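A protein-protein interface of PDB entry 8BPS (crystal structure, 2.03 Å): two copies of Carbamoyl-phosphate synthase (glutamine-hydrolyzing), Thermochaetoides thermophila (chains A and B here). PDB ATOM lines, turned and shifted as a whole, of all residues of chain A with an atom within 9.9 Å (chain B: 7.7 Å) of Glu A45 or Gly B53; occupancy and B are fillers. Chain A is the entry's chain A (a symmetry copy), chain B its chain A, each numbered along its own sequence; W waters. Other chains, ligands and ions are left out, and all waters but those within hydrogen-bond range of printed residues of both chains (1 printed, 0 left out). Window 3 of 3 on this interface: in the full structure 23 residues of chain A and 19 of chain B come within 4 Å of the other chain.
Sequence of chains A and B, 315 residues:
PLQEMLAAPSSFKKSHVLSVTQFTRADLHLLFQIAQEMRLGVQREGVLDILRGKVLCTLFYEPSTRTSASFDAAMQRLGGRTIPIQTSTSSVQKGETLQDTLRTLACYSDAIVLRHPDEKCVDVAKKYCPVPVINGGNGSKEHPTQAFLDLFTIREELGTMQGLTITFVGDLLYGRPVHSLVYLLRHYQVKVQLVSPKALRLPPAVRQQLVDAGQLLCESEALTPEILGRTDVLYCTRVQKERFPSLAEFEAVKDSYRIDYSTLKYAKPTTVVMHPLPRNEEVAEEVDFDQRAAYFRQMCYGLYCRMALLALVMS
OE1 of Gln A76 is in hydrogen-bond range of NH1 of Arg B81. NH2 of Arg B81 lies within hydrogen-bond range of O of Gly A79 (3.2 Å). OD2 of Asp B110 is in salt-bridge range of NH2 of Arg A77 (3.2 Å).
O of Lys B54 is in hydrogen-bond range of N of Arg B81 (3.0 Å). The backbone carbonyl oxygen of Val B55 lies within hydrogen-bond range of the backbone NH of Asp B110, 2.7 Å away. OE2 of Glu A45 is in salt-bridge range of NH2 of Arg A44 (2.7 Å). NH1 of Arg A77 sits at hydrogen-bond distance from O of Gly A46 (2.9 Å). The backbone NH (N) of Leu A48 sits at hydrogen-bond distance from the backbone carbonyl oxygen (O) of Arg A77 (2.8 Å). N of Gly A79 sits close to O of Leu A48, 3.3 Å away.
CA of Gly B53 touches O of Glu A45 (3.7 Å). Gly B53 touches Gly A46. Arg B52 touches Val A47 (O to CG2, 3.7 Å). Gly B53 touches Val A47. NH1 of Arg A77 touches O of Gly B53, at 3.99 Å. NH2 of Arg A77 touches CG2 of Val B55, at 3.5 Å.
Glu A45 touches just one residue of chain B: Gly B53. Of the printed residues of chain A, Gly B53 touches Glu A45, Gly A46, Val A47 and Arg A77. Printed residues of chain A within 4 Å of Val B55: Arg A77 (3.5 Å). Printed residues of chain A within 4 Å of Arg B52: Val A47 (3.7 Å). Printed residues of chain A within 4 Å of Arg B81: Gln A76 (2.8 Å) and Gly A79 (3.2 Å). Printed residues of chain A within 4 Å of Asp B110: Arg A77 (3.2 Å). Met A38 touches none of the printed residues of chain B. Gly B80 touches none of the printed residues of chain A. The nearest printed residue of chain B that does not touch Val A47 is Arg B81 (4.2 Å).
Printed residues of chain B that touch a printed residue of chain A: Arg B52, Gly B53, Val B55, Arg B81 and Asp B110. Hydrophobic or aromatic side chains of chain B that line the printed part of chain A: Val B55. Among the printed residues, 9 pairs touch across the chains.
Positions printed for both chains: 49, 50, 52, 78 and 79. Of the 9 pairs that touch across the chains among the printed residues, none has its exchanged pair printed and touching as well.
Water W1 lies within hydrogen-bond range of NH1 of Arg A77, O of Gly B53 and OD2 of Asp B110.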
ATOM      1  N   PRO A   1      10.185   7.059  -9.546  1.00  0.00           N
ATOM      2  CA  PRO A   1      11.479   7.563 -10.037  1.00  0.00           C
ATOM      3  C   PRO A   1      11.968   8.791  -9.262  1.00  0.00           C
ATOM      4  O   PRO A   1      13.153   8.846  -8.905  1.00  0.00           O
ATOM      5  CB  PRO A   1      11.190   7.927 -11.497  1.00  0.00           C
ATOM      6  CG  PRO A   1       9.728   8.298 -11.497  1.00  0.00           C
ATOM      7  CD  PRO A   1       9.071   7.399 -10.453  1.00  0.00           C
ATOM      8  N   LEU A   2      11.076   9.765  -9.028  1.00  0.00           N
ATOM      9  CA  LEU A   2      11.417  10.863  -8.127  1.00  0.00           C
ATOM     10  C   LEU A   2      11.827  10.321  -6.760  1.00  0.00           C
ATOM     11  O   LEU A   2      12.799  10.789  -6.153  1.00  0.00           O
ATOM     12  CB  LEU A   2      10.237  11.828  -7.998  1.00  0.00           C
ATOM     13  N   GLN A   3      11.116   9.298  -6.282  1.00  0.00           N
ATOM     14  CA  GLN A   3      11.454   8.658  -5.012  1.00  0.00           C
ATOM     15  C   GLN A   3      12.892   8.136  -5.007  1.00  0.00           C
ATOM     16  O   GLN A   3      13.606   8.266  -4.004  1.00  0.00           O
ATOM     17  CB  GLN A   3      10.485   7.505  -4.746  1.00  0.00           C
ATOM     18  CG  GLN A   3      10.126   6.736  -6.010  1.00  0.00           C
ATOM     19  CD  GLN A   3       8.747   6.087  -5.932  1.00  0.00           C
ATOM     20  OE1 GLN A   3       7.976   6.346  -4.999  1.00  0.00           O
ATOM     21  NE2 GLN A   3       8.429   5.240  -6.912  1.00  0.00           N
ATOM     22  N   GLU A  37      11.440  15.938 -12.963  1.00  0.00           N
ATOM     23  CA  GLU A  37      10.329  15.094 -12.530  1.00  0.00           C
ATOM     24  C   GLU A  37       9.276  15.881 -11.760  1.00  0.00           C
ATOM     25  O   GLU A  37       8.085  15.541 -11.836  1.00  0.00           O
ATOM     26  CB  GLU A  37      10.825  13.959 -11.649  1.00  0.00           C
ATOM     27  CG  GLU A  37      11.570  12.894 -12.400  1.00  0.00           C
ATOM     28  CD  GLU A  37      10.688  12.165 -13.391  1.00  0.00           C
ATOM     29  OE1 GLU A  37       9.607  11.674 -12.981  1.00  0.00           O
ATOM     30  OE2 GLU A  37      11.081  12.094 -14.580  1.00  0.00           O
ATOM     31  N   MET A  38       9.685  16.903 -10.998  1.00  0.00           N
ATOM     32  CA  MET A  38       8.706  17.713 -10.296  1.00  0.00           C
ATOM     33  C   MET A  38       7.714  18.299 -11.284  1.00  0.00           C
ATOM     34  O   MET A  38       6.504  18.325 -11.026  1.00  0.00           O
ATOM     35  CB  MET A  38       9.399  18.828  -9.499  1.00  0.00           C
ATOM     36  CG  MET A  38      10.225  18.322  -8.317  1.00  0.00           C
ATOM     37  SD  MET A  38       9.149  17.515  -7.110  1.00  0.00           S
ATOM     38  CE  MET A  38      10.334  16.937  -5.905  1.00  0.00           C
ATOM     39  N   ARG A  39       8.212  18.759 -12.434  1.00  0.00           N
ATOM     40  CA  ARG A  39       7.333  19.323 -13.455  1.00  0.00           C
ATOM     41  C   ARG A  39       6.371  18.269 -13.987  1.00  0.00           C
ATOM     42  O   ARG A  39       5.176  18.539 -14.157  1.00  0.00           O
ATOM     43  CB  ARG A  39       8.155  19.915 -14.607  1.00  0.00           C
ATOM     44  CG  ARG A  39       7.326  20.531 -15.726  1.00  0.00           C
ATOM     45  CD  ARG A  39       8.135  20.886 -16.977  1.00  0.00           C
ATOM     46  NE  ARG A  39       9.370  20.118 -17.081  1.00  0.00           N
ATOM     47  CZ  ARG A  39      10.488  20.555 -17.640  1.00  0.00           C
ATOM     48  NH1 ARG A  39      10.565  21.757 -18.186  1.00  0.00           N
ATOM     49  NH2 ARG A  39      11.557  19.763 -17.652  1.00  0.00           N
ATOM     50  N   LEU A  40       6.874  17.062 -14.275  1.00  0.00           N
ATOM     51  CA  LEU A  40       5.980  16.010 -14.757  1.00  0.00           C
ATOM     52  C   LEU A  40       4.926  15.685 -13.709  1.00  0.00           C
ATOM     53  O   LEU A  40       3.738  15.554 -14.029  1.00  0.00           O
ATOM     54  CB  LEU A  40       6.775  14.760 -15.121  1.00  0.00           C
ATOM     55  CG  LEU A  40       7.836  14.994 -16.191  1.00  0.00           C
ATOM     56  CD1 LEU A  40       8.526  13.677 -16.543  1.00  0.00           C
ATOM     57  CD2 LEU A  40       7.289  15.619 -17.472  1.00  0.00           C
ATOM     58  N   GLY A  41       5.338  15.585 -12.442  1.00  0.00           N
ATOM     59  CA  GLY A  41       4.382  15.286 -11.395  1.00  0.00           C
ATOM     60  C   GLY A  41       3.302  16.345 -11.289  1.00  0.00           C
ATOM     61  O   GLY A  41       2.113  16.031 -11.183  1.00  0.00           O
ATOM     62  N   VAL A  42       3.707  17.620 -11.314  1.00  0.00           N
ATOM     63  CA  VAL A  42       2.742  18.706 -11.213  1.00  0.00           C
ATOM     64  C   VAL A  42       1.763  18.677 -12.382  1.00  0.00           C
ATOM     65  O   VAL A  42       0.554  18.881 -12.206  1.00  0.00           O
ATOM     66  CB  VAL A  42       3.473  20.060 -11.124  1.00  0.00           C
ATOM     67  CG1 VAL A  42       2.484  21.199 -11.330  1.00  0.00           C
ATOM     68  CG2 VAL A  42       4.199  20.212  -9.775  1.00  0.00           C
ATOM     69  N   GLN A  43       2.266  18.453 -13.593  1.00  0.00           N
ATOM     70  CA  GLN A  43       1.378  18.338 -14.746  1.00  0.00           C
ATOM     71  C   GLN A  43       0.337  17.237 -14.541  1.00  0.00           C
ATOM     72  O   GLN A  43      -0.821  17.395 -14.948  1.00  0.00           O
ATOM     73  CB  GLN A  43       2.218  18.097 -16.003  1.00  0.00           C
ATOM     74  CG  GLN A  43       3.164  19.272 -16.319  1.00  0.00           C
ATOM     75  CD  GLN A  43       4.077  19.018 -17.505  1.00  0.00           C
ATOM     76  OE1 GLN A  43       4.312  17.871 -17.880  1.00  0.00           O
ATOM     77  NE2 GLN A  43       4.615  20.092 -18.090  1.00  0.00           N
ATOM     78  N   ARG A  44       0.712  16.145 -13.875  1.00  0.00           N
ATOM     79  CA  ARG A  44      -0.199  15.025 -13.678  1.00  0.00           C
ATOM     80  C   ARG A  44      -1.110  15.191 -12.459  1.00  0.00           C
ATOM     81  O   ARG A  44      -2.311  14.909 -12.555  1.00  0.00           O
ATOM     82  CB  ARG A  44       0.612  13.731 -13.538  1.00  0.00           C
ATOM     83  CG  ARG A  44       1.475  13.374 -14.756  1.00  0.00           C
ATOM     84  CD  ARG A  44       2.480  12.232 -14.437  1.00  0.00           C
ATOM     85  NE  ARG A  44       2.206  11.598 -13.147  1.00  0.00           N
ATOM     86  CZ  ARG A  44       3.101  11.381 -12.187  1.00  0.00           C
ATOM     87  NH1 ARG A  44       4.385  11.672 -12.348  1.00  0.00           N
ATOM     88  NH2 ARG A  44       2.695  10.862 -11.029  1.00  0.00           N
ATOM     89  N   GLU A  45      -0.559  15.613 -11.306  1.00  0.00           N
ATOM     90  CA  GLU A  45      -1.300  15.615 -10.059  1.00  0.00           C
ATOM     91  C   GLU A  45      -1.524  16.989  -9.452  1.00  0.00           C
ATOM     92  O   GLU A  45      -2.345  17.100  -8.530  1.00  0.00           O
ATOM     93  CB  GLU A  45      -0.600  14.751  -8.996  1.00  0.00           C
ATOM     94  CG  GLU A  45      -0.193  13.347  -9.407  1.00  0.00           C
ATOM     95  CD  GLU A  45       0.829  12.736  -8.443  1.00  0.00           C
ATOM     96  OE1 GLU A  45       0.523  12.608  -7.235  1.00  0.00           O
ATOM     97  OE2 GLU A  45       1.947  12.388  -8.883  1.00  0.00           O
ATOM     98  N   GLY A  46      -0.797  18.017  -9.890  1.00  0.00           N
ATOM     99  CA  GLY A  46      -0.994  19.362  -9.368  1.00  0.00           C
ATOM    100  C   GLY A  46      -0.340  19.566  -8.018  1.00  0.00           C
ATOM    101  O   GLY A  46       0.567  20.398  -7.868  1.00  0.00           O
ATOM    102  N   VAL A  47      -0.793  18.799  -7.026  1.00  0.00           N
ATOM    103  CA  VAL A  47      -0.205  18.799  -5.693  1.00  0.00           C
ATOM    104  C   VAL A  47       0.269  17.382  -5.400  1.00  0.00           C
ATOM    105  O   VAL A  47      -0.532  16.442  -5.396  1.00  0.00           O
ATOM    106  CB  VAL A  47      -1.198  19.279  -4.628  1.00  0.00           C
ATOM    107  CG1 VAL A  47      -0.642  19.020  -3.242  1.00  0.00           C
ATOM    108  CG2 VAL A  47      -1.499  20.749  -4.834  1.00  0.00           C
ATOM    109  N   LEU A  48       1.561  17.235  -5.137  1.00  0.00           N
ATOM    110  CA  LEU A  48       2.169  15.935  -4.911  1.00  0.00           C
ATOM    111  C   LEU A  48       2.148  15.561  -3.423  1.00  0.00           C
ATOM    112  O   LEU A  48       1.657  16.295  -2.561  1.00  0.00           O
ATOM    113  CB  LEU A  48       3.598  15.942  -5.444  1.00  0.00           C
ATOM    114  CG  LEU A  48       3.814  16.366  -6.902  1.00  0.00           C
ATOM    115  CD1 LEU A  48       5.303  16.275  -7.267  1.00  0.00           C
ATOM    116  CD2 LEU A  48       2.979  15.519  -7.848  1.00  0.00           C
ATOM    117  N   ASP A  49       2.713  14.399  -3.121  1.00  0.00           N
ATOM    118  CA  ASP A  49       2.742  13.857  -1.769  1.00  0.00           C
ATOM    119  C   ASP A  49       4.191  13.478  -1.438  1.00  0.00           C
ATOM    120  O   ASP A  49       4.535  12.289  -1.378  1.00  0.00           O
ATOM    121  CB  ASP A  49       1.807  12.640  -1.656  1.00  0.00           C
ATOM    122  CG  ASP A  49       1.926  11.935  -0.331  1.00  0.00           C
ATOM    123  OD1 ASP A  49       1.179  10.953  -0.123  1.00  0.00           O
ATOM    124  OD2 ASP A  49       2.753  12.361   0.510  1.00  0.00           O
ATOM    125  N   ILE A  50       5.037  14.480  -1.276  1.00  0.00           N
ATOM    126  CA  ILE A  50       6.448  14.300  -0.970  1.00  0.00           C
ATOM    127  C   ILE A  50       6.773  14.819   0.421  1.00  0.00           C
ATOM    128  O   ILE A  50       7.457  14.155   1.197  1.00  0.00           O
ATOM    129  CB  ILE A  50       7.336  15.002  -2.026  1.00  0.00           C
ATOM    130  CG1 ILE A  50       7.318  14.321  -3.385  1.00  0.00           C
ATOM    131  CG2 ILE A  50       8.806  15.079  -1.582  1.00  0.00           C
ATOM    132  CD1 ILE A  50       5.999  14.316  -4.030  1.00  0.00           C
ATOM    133  N   ARG A  52       4.403  15.900   2.860  1.00  0.00           N
ATOM    134  CA  ARG A  52       3.071  16.083   3.434  1.00  0.00           C
ATOM    135  C   ARG A  52       3.109  16.480   4.909  1.00  0.00           C
ATOM    136  O   ARG A  52       2.244  17.238   5.371  1.00  0.00           O
ATOM    137  CB  ARG A  52       2.267  14.793   3.277  1.00  0.00           C
ATOM    138  CG  ARG A  52       1.174  14.817   2.229  1.00  0.00           C
ATOM    139  CD  ARG A  52       0.082  13.787   2.585  1.00  0.00           C
ATOM    140  NE  ARG A  52      -0.362  13.976   3.964  1.00  0.00           N
ATOM    141  CZ  ARG A  52      -0.207  13.095   4.946  1.00  0.00           C
ATOM    142  NH1 ARG A  52       0.228  11.868   4.715  1.00  0.00           N
ATOM    143  NH2 ARG A  52      -0.481  13.463   6.195  1.00  0.00           N
ATOM    144  N   ALA A  73       4.407  28.338  -3.223  1.00  0.00           N
ATOM    145  CA  ALA A  73       3.771  27.426  -4.166  1.00  0.00           C
ATOM    146  C   ALA A  73       4.559  26.126  -4.313  1.00  0.00           C
ATOM    147  O   ALA A  73       3.964  25.045  -4.436  1.00  0.00           O
ATOM    148  CB  ALA A  73       3.610  28.123  -5.510  1.00  0.00           C
ATOM    149  N   GLN A  76       3.812  24.029  -1.180  1.00  0.00           N
ATOM    150  CA  GLN A  76       2.454  23.497  -1.180  1.00  0.00           C
ATOM    151  C   GLN A  76       2.256  22.482  -2.295  1.00  0.00           C
ATOM    152  O   GLN A  76       1.557  21.484  -2.098  1.00  0.00           O
ATOM    153  CB  GLN A  76       1.431  24.631  -1.286  1.00  0.00           C
ATOM    154  CG  GLN A  76       1.460  25.591  -0.079  1.00  0.00           C
ATOM    155  CD  GLN A  76       0.138  26.264   0.187  1.00  0.00           C
ATOM    156  OE1 GLN A  76      -0.876  25.589   0.419  1.00  0.00           O
ATOM    157  NE2 GLN A  76       0.122  27.600   0.134  1.00  0.00           N
ATOM    158  N   ARG A  77       2.882  22.679  -3.456  1.00  0.00           N
ATOM    159  CA  ARG A  77       2.750  21.653  -4.493  1.00  0.00           C
ATOM    160  C   ARG A  77       3.536  20.391  -4.163  1.00  0.00           C
ATOM    161  O   ARG A  77       3.318  19.351  -4.809  1.00  0.00           O
ATOM    162  CB  ARG A  77       3.177  22.219  -5.848  1.00  0.00           C
ATOM    163  CG  ARG A  77       2.140  23.200  -6.425  1.00  0.00           C
ATOM    164  CD  ARG A  77       2.499  23.635  -7.846  1.00  0.00           C
ATOM    165  NE  ARG A  77       1.566  24.604  -8.401  1.00  0.00           N
ATOM    166  CZ  ARG A  77       0.403  24.291  -8.955  1.00  0.00           C
ATOM    167  NH1 ARG A  77       0.001  23.030  -9.047  1.00  0.00           N
ATOM    168  NH2 ARG A  77      -0.376  25.266  -9.422  1.00  0.00           N
ATOM    169  N   LEU A  78       4.431  20.439  -3.168  1.00  0.00           N
ATOM    170  CA  LEU A  78       5.019  19.202  -2.662  1.00  0.00           C
ATOM    171  C   LEU A  78       4.114  18.516  -1.647  1.00  0.00           C
ATOM    172  O   LEU A  78       4.479  17.452  -1.126  1.00  0.00           O
ATOM    173  CB  LEU A  78       6.403  19.476  -2.038  1.00  0.00           C
ATOM    174  CG  LEU A  78       7.519  19.828  -3.019  1.00  0.00           C
ATOM    175  CD1 LEU A  78       8.663  20.474  -2.254  1.00  0.00           C
ATOM    176  CD2 LEU A  78       8.028  18.602  -3.768  1.00  0.00           C
ATOM    177  N   GLY A  79       2.944  19.097  -1.365  1.00  0.00           N
ATOM    178  CA  GLY A  79       2.047  18.617  -0.335  1.00  0.00           C
ATOM    179  C   GLY A  79       2.361  19.109   1.062  1.00  0.00           C
ATOM    180  O   GLY A  79       1.641  18.754   1.998  1.00  0.00           O
ATOM    181  N   MET A 307      10.925  23.346  -5.902  1.00  0.00           N
ATOM    182  CA  MET A 307      10.318  22.104  -5.453  1.00  0.00           C
ATOM    183  C   MET A 307      11.392  21.050  -5.191  1.00  0.00           C
ATOM    184  O   MET A 307      11.400  20.399  -4.138  1.00  0.00           O
ATOM    185  CB  MET A 307       9.308  21.606  -6.488  1.00  0.00           C
ATOM    186  CG  MET A 307       7.965  22.330  -6.378  1.00  0.00           C
ATOM    187  SD  MET A 307       6.757  21.796  -7.616  1.00  0.00           S
ATOM    188  CE  MET A 307       6.115  20.353  -6.759  1.00  0.00           C
ATOM    189  N   ASP B  49     -13.141  17.528  -1.253  1.00  0.00           N
ATOM    190  CA  ASP B  49     -12.088  16.994  -2.108  1.00  0.00           C
ATOM    191  C   ASP B  49     -12.514  17.186  -3.569  1.00  0.00           C
ATOM    192  O   ASP B  49     -12.866  16.218  -4.257  1.00  0.00           O
ATOM    193  CB  ASP B  49     -11.840  15.508  -1.790  1.00  0.00           C
ATOM    194  CG  ASP B  49     -10.884  14.858  -2.756  1.00  0.00           C
ATOM    195  OD1 ASP B  49     -10.585  13.659  -2.563  1.00  0.00           O
ATOM    196  OD2 ASP B  49     -10.420  15.540  -3.700  1.00  0.00           O
ATOM    197  N   ILE B  50     -12.529  18.430  -4.014  1.00  0.00           N
ATOM    198  CA  ILE B  50     -12.918  18.792  -5.369  1.00  0.00           C
ATOM    199  C   ILE B  50     -11.734  19.351  -6.143  1.00  0.00           C
ATOM    200  O   ILE B  50     -11.498  18.972  -7.288  1.00  0.00           O
ATOM    201  CB  ILE B  50     -14.079  19.816  -5.354  1.00  0.00           C
ATOM    202  CG1 ILE B  50     -15.405  19.226  -4.897  1.00  0.00           C
ATOM    203  CG2 ILE B  50     -14.318  20.435  -6.742  1.00  0.00           C
ATOM    204  CD1 ILE B  50     -15.390  18.740  -3.512  1.00  0.00           C
ATOM    205  N   LEU B  51     -10.977  20.251  -5.525  1.00  0.00           N
ATOM    206  CA  LEU B  51      -9.847  20.935  -6.153  1.00  0.00           C
ATOM    207  C   LEU B  51      -8.535  20.624  -5.428  1.00  0.00           C
ATOM    208  O   LEU B  51      -7.678  21.476  -5.259  1.00  0.00           O
ATOM    209  CB  LEU B  51     -10.084  22.444  -6.205  1.00  0.00           C
ATOM    210  CG  LEU B  51     -11.262  22.919  -7.046  1.00  0.00           C
ATOM    211  CD1 LEU B  51     -11.292  24.468  -7.055  1.00  0.00           C
ATOM    212  CD2 LEU B  51     -11.212  22.346  -8.472  1.00  0.00           C
ATOM    213  N   ARG B  52      -8.337  19.360  -5.053  1.00  0.00           N
ATOM    214  CA  ARG B  52      -7.213  19.001  -4.191  1.00  0.00           C
ATOM    215  C   ARG B  52      -5.856  19.332  -4.811  1.00  0.00           C
ATOM    216  O   ARG B  52      -4.913  19.685  -4.089  1.00  0.00           O
ATOM    217  CB  ARG B  52      -7.272  17.508  -3.871  1.00  0.00           C
ATOM    218  CG  ARG B  52      -7.705  17.146  -2.467  1.00  0.00           C
ATOM    219  CD  ARG B  52      -7.135  15.766  -2.080  1.00  0.00           C
ATOM    220  NE  ARG B  52      -5.696  15.724  -2.326  1.00  0.00           N
ATOM    221  CZ  ARG B  52      -5.094  14.937  -3.212  1.00  0.00           C
ATOM    222  NH1 ARG B  52      -5.748  13.978  -3.846  1.00  0.00           N
ATOM    223  NH2 ARG B  52      -3.804  15.130  -3.478  1.00  0.00           N
ATOM    224  N   GLY B  53      -5.723  19.227  -6.120  1.00  0.00           N
ATOM    225  CA  GLY B  53      -4.451  19.502  -6.754  1.00  0.00           C
ATOM    226  C   GLY B  53      -4.319  20.886  -7.338  1.00  0.00           C
ATOM    227  O   GLY B  53      -3.377  21.120  -8.102  1.00  0.00           O
ATOM    228  N   LYS B  54      -5.210  21.811  -6.996  1.00  0.00           N
ATOM    229  CA  LYS B  54      -5.225  23.140  -7.591  1.00  0.00           C
ATOM    230  C   LYS B  54      -4.744  24.195  -6.594  1.00  0.00           C
ATOM    231  O   LYS B  54      -4.873  24.042  -5.370  1.00  0.00           O
ATOM    232  CB  LYS B  54      -6.632  23.510  -8.073  1.00  0.00           C
ATOM    233  CG  LYS B  54      -7.253  22.541  -9.067  1.00  0.00           C
ATOM    234  CD  LYS B  54      -6.320  22.281 -10.232  1.00  0.00           C
ATOM    235  CE  LYS B  54      -7.047  21.587 -11.373  1.00  0.00           C
ATOM    236  NZ  LYS B  54      -6.143  21.477 -12.577  1.00  0.00           N
ATOM    237  N   VAL B  55      -4.218  25.291  -7.144  1.00  0.00           N
ATOM    238  CA  VAL B  55      -3.636  26.379  -6.359  1.00  0.00           C
ATOM    239  C   VAL B  55      -4.230  27.696  -6.841  1.00  0.00           C
ATOM    240  O   VAL B  55      -4.189  27.993  -8.037  1.00  0.00           O
ATOM    241  CB  VAL B  55      -2.101  26.400  -6.486  1.00  0.00           C
ATOM    242  CG1 VAL B  55      -1.484  27.512  -5.641  1.00  0.00           C
ATOM    243  CG2 VAL B  55      -1.525  25.011  -6.154  1.00  0.00           C
ATOM    244  N   MET B  75     -11.647  28.374  -1.584  1.00  0.00           N
ATOM    245  CA  MET B  75     -10.649  27.517  -2.216  1.00  0.00           C
ATOM    246  C   MET B  75     -10.194  26.410  -1.254  1.00  0.00           C
ATOM    247  O   MET B  75     -10.145  25.223  -1.617  1.00  0.00           O
ATOM    248  CB  MET B  75      -9.445  28.362  -2.663  1.00  0.00           C
ATOM    249  CG  MET B  75      -8.470  27.561  -3.493  1.00  0.00           C
ATOM    250  SD  MET B  75      -9.200  26.936  -5.037  1.00  0.00           S
ATOM    251  CE  MET B  75      -7.730  26.176  -5.772  1.00  0.00           C
ATOM    252  N   LEU B  78     -12.647  23.764  -0.699  1.00  0.00           N
ATOM    253  CA  LEU B  78     -12.727  22.830  -1.819  1.00  0.00           C
ATOM    254  C   LEU B  78     -11.589  21.816  -1.794  1.00  0.00           C
ATOM    255  O   LEU B  78     -11.521  20.956  -2.685  1.00  0.00           O
ATOM    256  CB  LEU B  78     -12.728  23.590  -3.160  1.00  0.00           C
ATOM    257  CG  LEU B  78     -13.999  24.376  -3.479  1.00  0.00           C
ATOM    258  CD1 LEU B  78     -13.694  25.384  -4.575  1.00  0.00           C
ATOM    259  CD2 LEU B  78     -15.137  23.464  -3.920  1.00  0.00           C
ATOM    260  N   GLY B  79     -10.707  21.896  -0.793  1.00  0.00           N
ATOM    261  CA  GLY B  79      -9.517  21.075  -0.717  1.00  0.00           C
ATOM    262  C   GLY B  79      -8.329  21.603  -1.494  1.00  0.00           C
ATOM    263  O   GLY B  79      -7.273  20.967  -1.476  1.00  0.00           O
ATOM    264  N   GLY B  80      -8.462  22.739  -2.176  1.00  0.00           N
ATOM    265  CA  GLY B  80      -7.351  23.338  -2.863  1.00  0.00           C
ATOM    266  C   GLY B  80      -6.423  24.083  -1.920  1.00  0.00           C
ATOM    267  O   GLY B  80      -6.598  24.100  -0.702  1.00  0.00           O
ATOM    268  N   ARG B  81      -5.421  24.718  -2.526  1.00  0.00           N
ATOM    269  CA  ARG B  81      -4.411  25.486  -1.828  1.00  0.00           C
ATOM    270  C   ARG B  81      -4.513  26.943  -2.237  1.00  0.00           C
ATOM    271  O   ARG B  81      -4.946  27.258  -3.351  1.00  0.00           O
ATOM    272  CB  ARG B  81      -2.991  24.985  -2.141  1.00  0.00           C
ATOM    273  CG  ARG B  81      -2.765  23.510  -1.876  1.00  0.00           C
ATOM    274  CD  ARG B  81      -2.980  23.148  -0.411  1.00  0.00           C
ATOM    275  NE  ARG B  81      -2.326  21.892  -0.055  1.00  0.00           N
ATOM    276  CZ  ARG B  81      -1.171  21.809   0.593  1.00  0.00           C
ATOM    277  NH1 ARG B  81      -0.488  22.901   0.940  1.00  0.00           N
ATOM    278  NH2 ARG B  81      -0.675  20.599   0.875  1.00  0.00           N
ATOM    279  N   ASP B 110      -3.066  28.151 -10.541  1.00  0.00           N
ATOM    280  CA  ASP B 110      -3.936  27.748 -11.640  1.00  0.00           C
ATOM    281  C   ASP B 110      -4.996  28.792 -11.924  1.00  0.00           C
ATOM    282  O   ASP B 110      -5.664  28.722 -12.962  1.00  0.00           O
ATOM    283  CB  ASP B 110      -4.575  26.382 -11.332  1.00  0.00           C
ATOM    284  CG  ASP B 110      -3.527  25.334 -10.944  1.00  0.00           C
ATOM    285  OD1 ASP B 110      -2.662  25.045 -11.800  1.00  0.00           O
ATOM    286  OD2 ASP B 110      -3.546  24.818  -9.801  1.00  0.00           O
ATOM    287  N   MET B 314     -11.985  25.906 -12.342  1.00  0.00           N
ATOM    288  CA  MET B 314     -10.720  25.193 -12.242  1.00  0.00           C
ATOM    289  C   MET B 314     -10.864  23.680 -12.341  1.00  0.00           C
ATOM    290  O   MET B 314      -9.853  22.994 -12.466  1.00  0.00           O
ATOM    291  CB  MET B 314     -10.036  25.536 -10.911  1.00  0.00           C
ATOM    292  CG  MET B 314     -10.172  26.999 -10.503  1.00  0.00           C
ATOM    293  SD  MET B 314      -9.103  27.518  -9.134  1.00  0.00           S
ATOM    294  CE  MET B 314      -7.600  26.662  -9.589  1.00  0.00           C
HETATM  295  O   HOH W   1      -2.251  22.402 -10.278  1.00  0.00           O
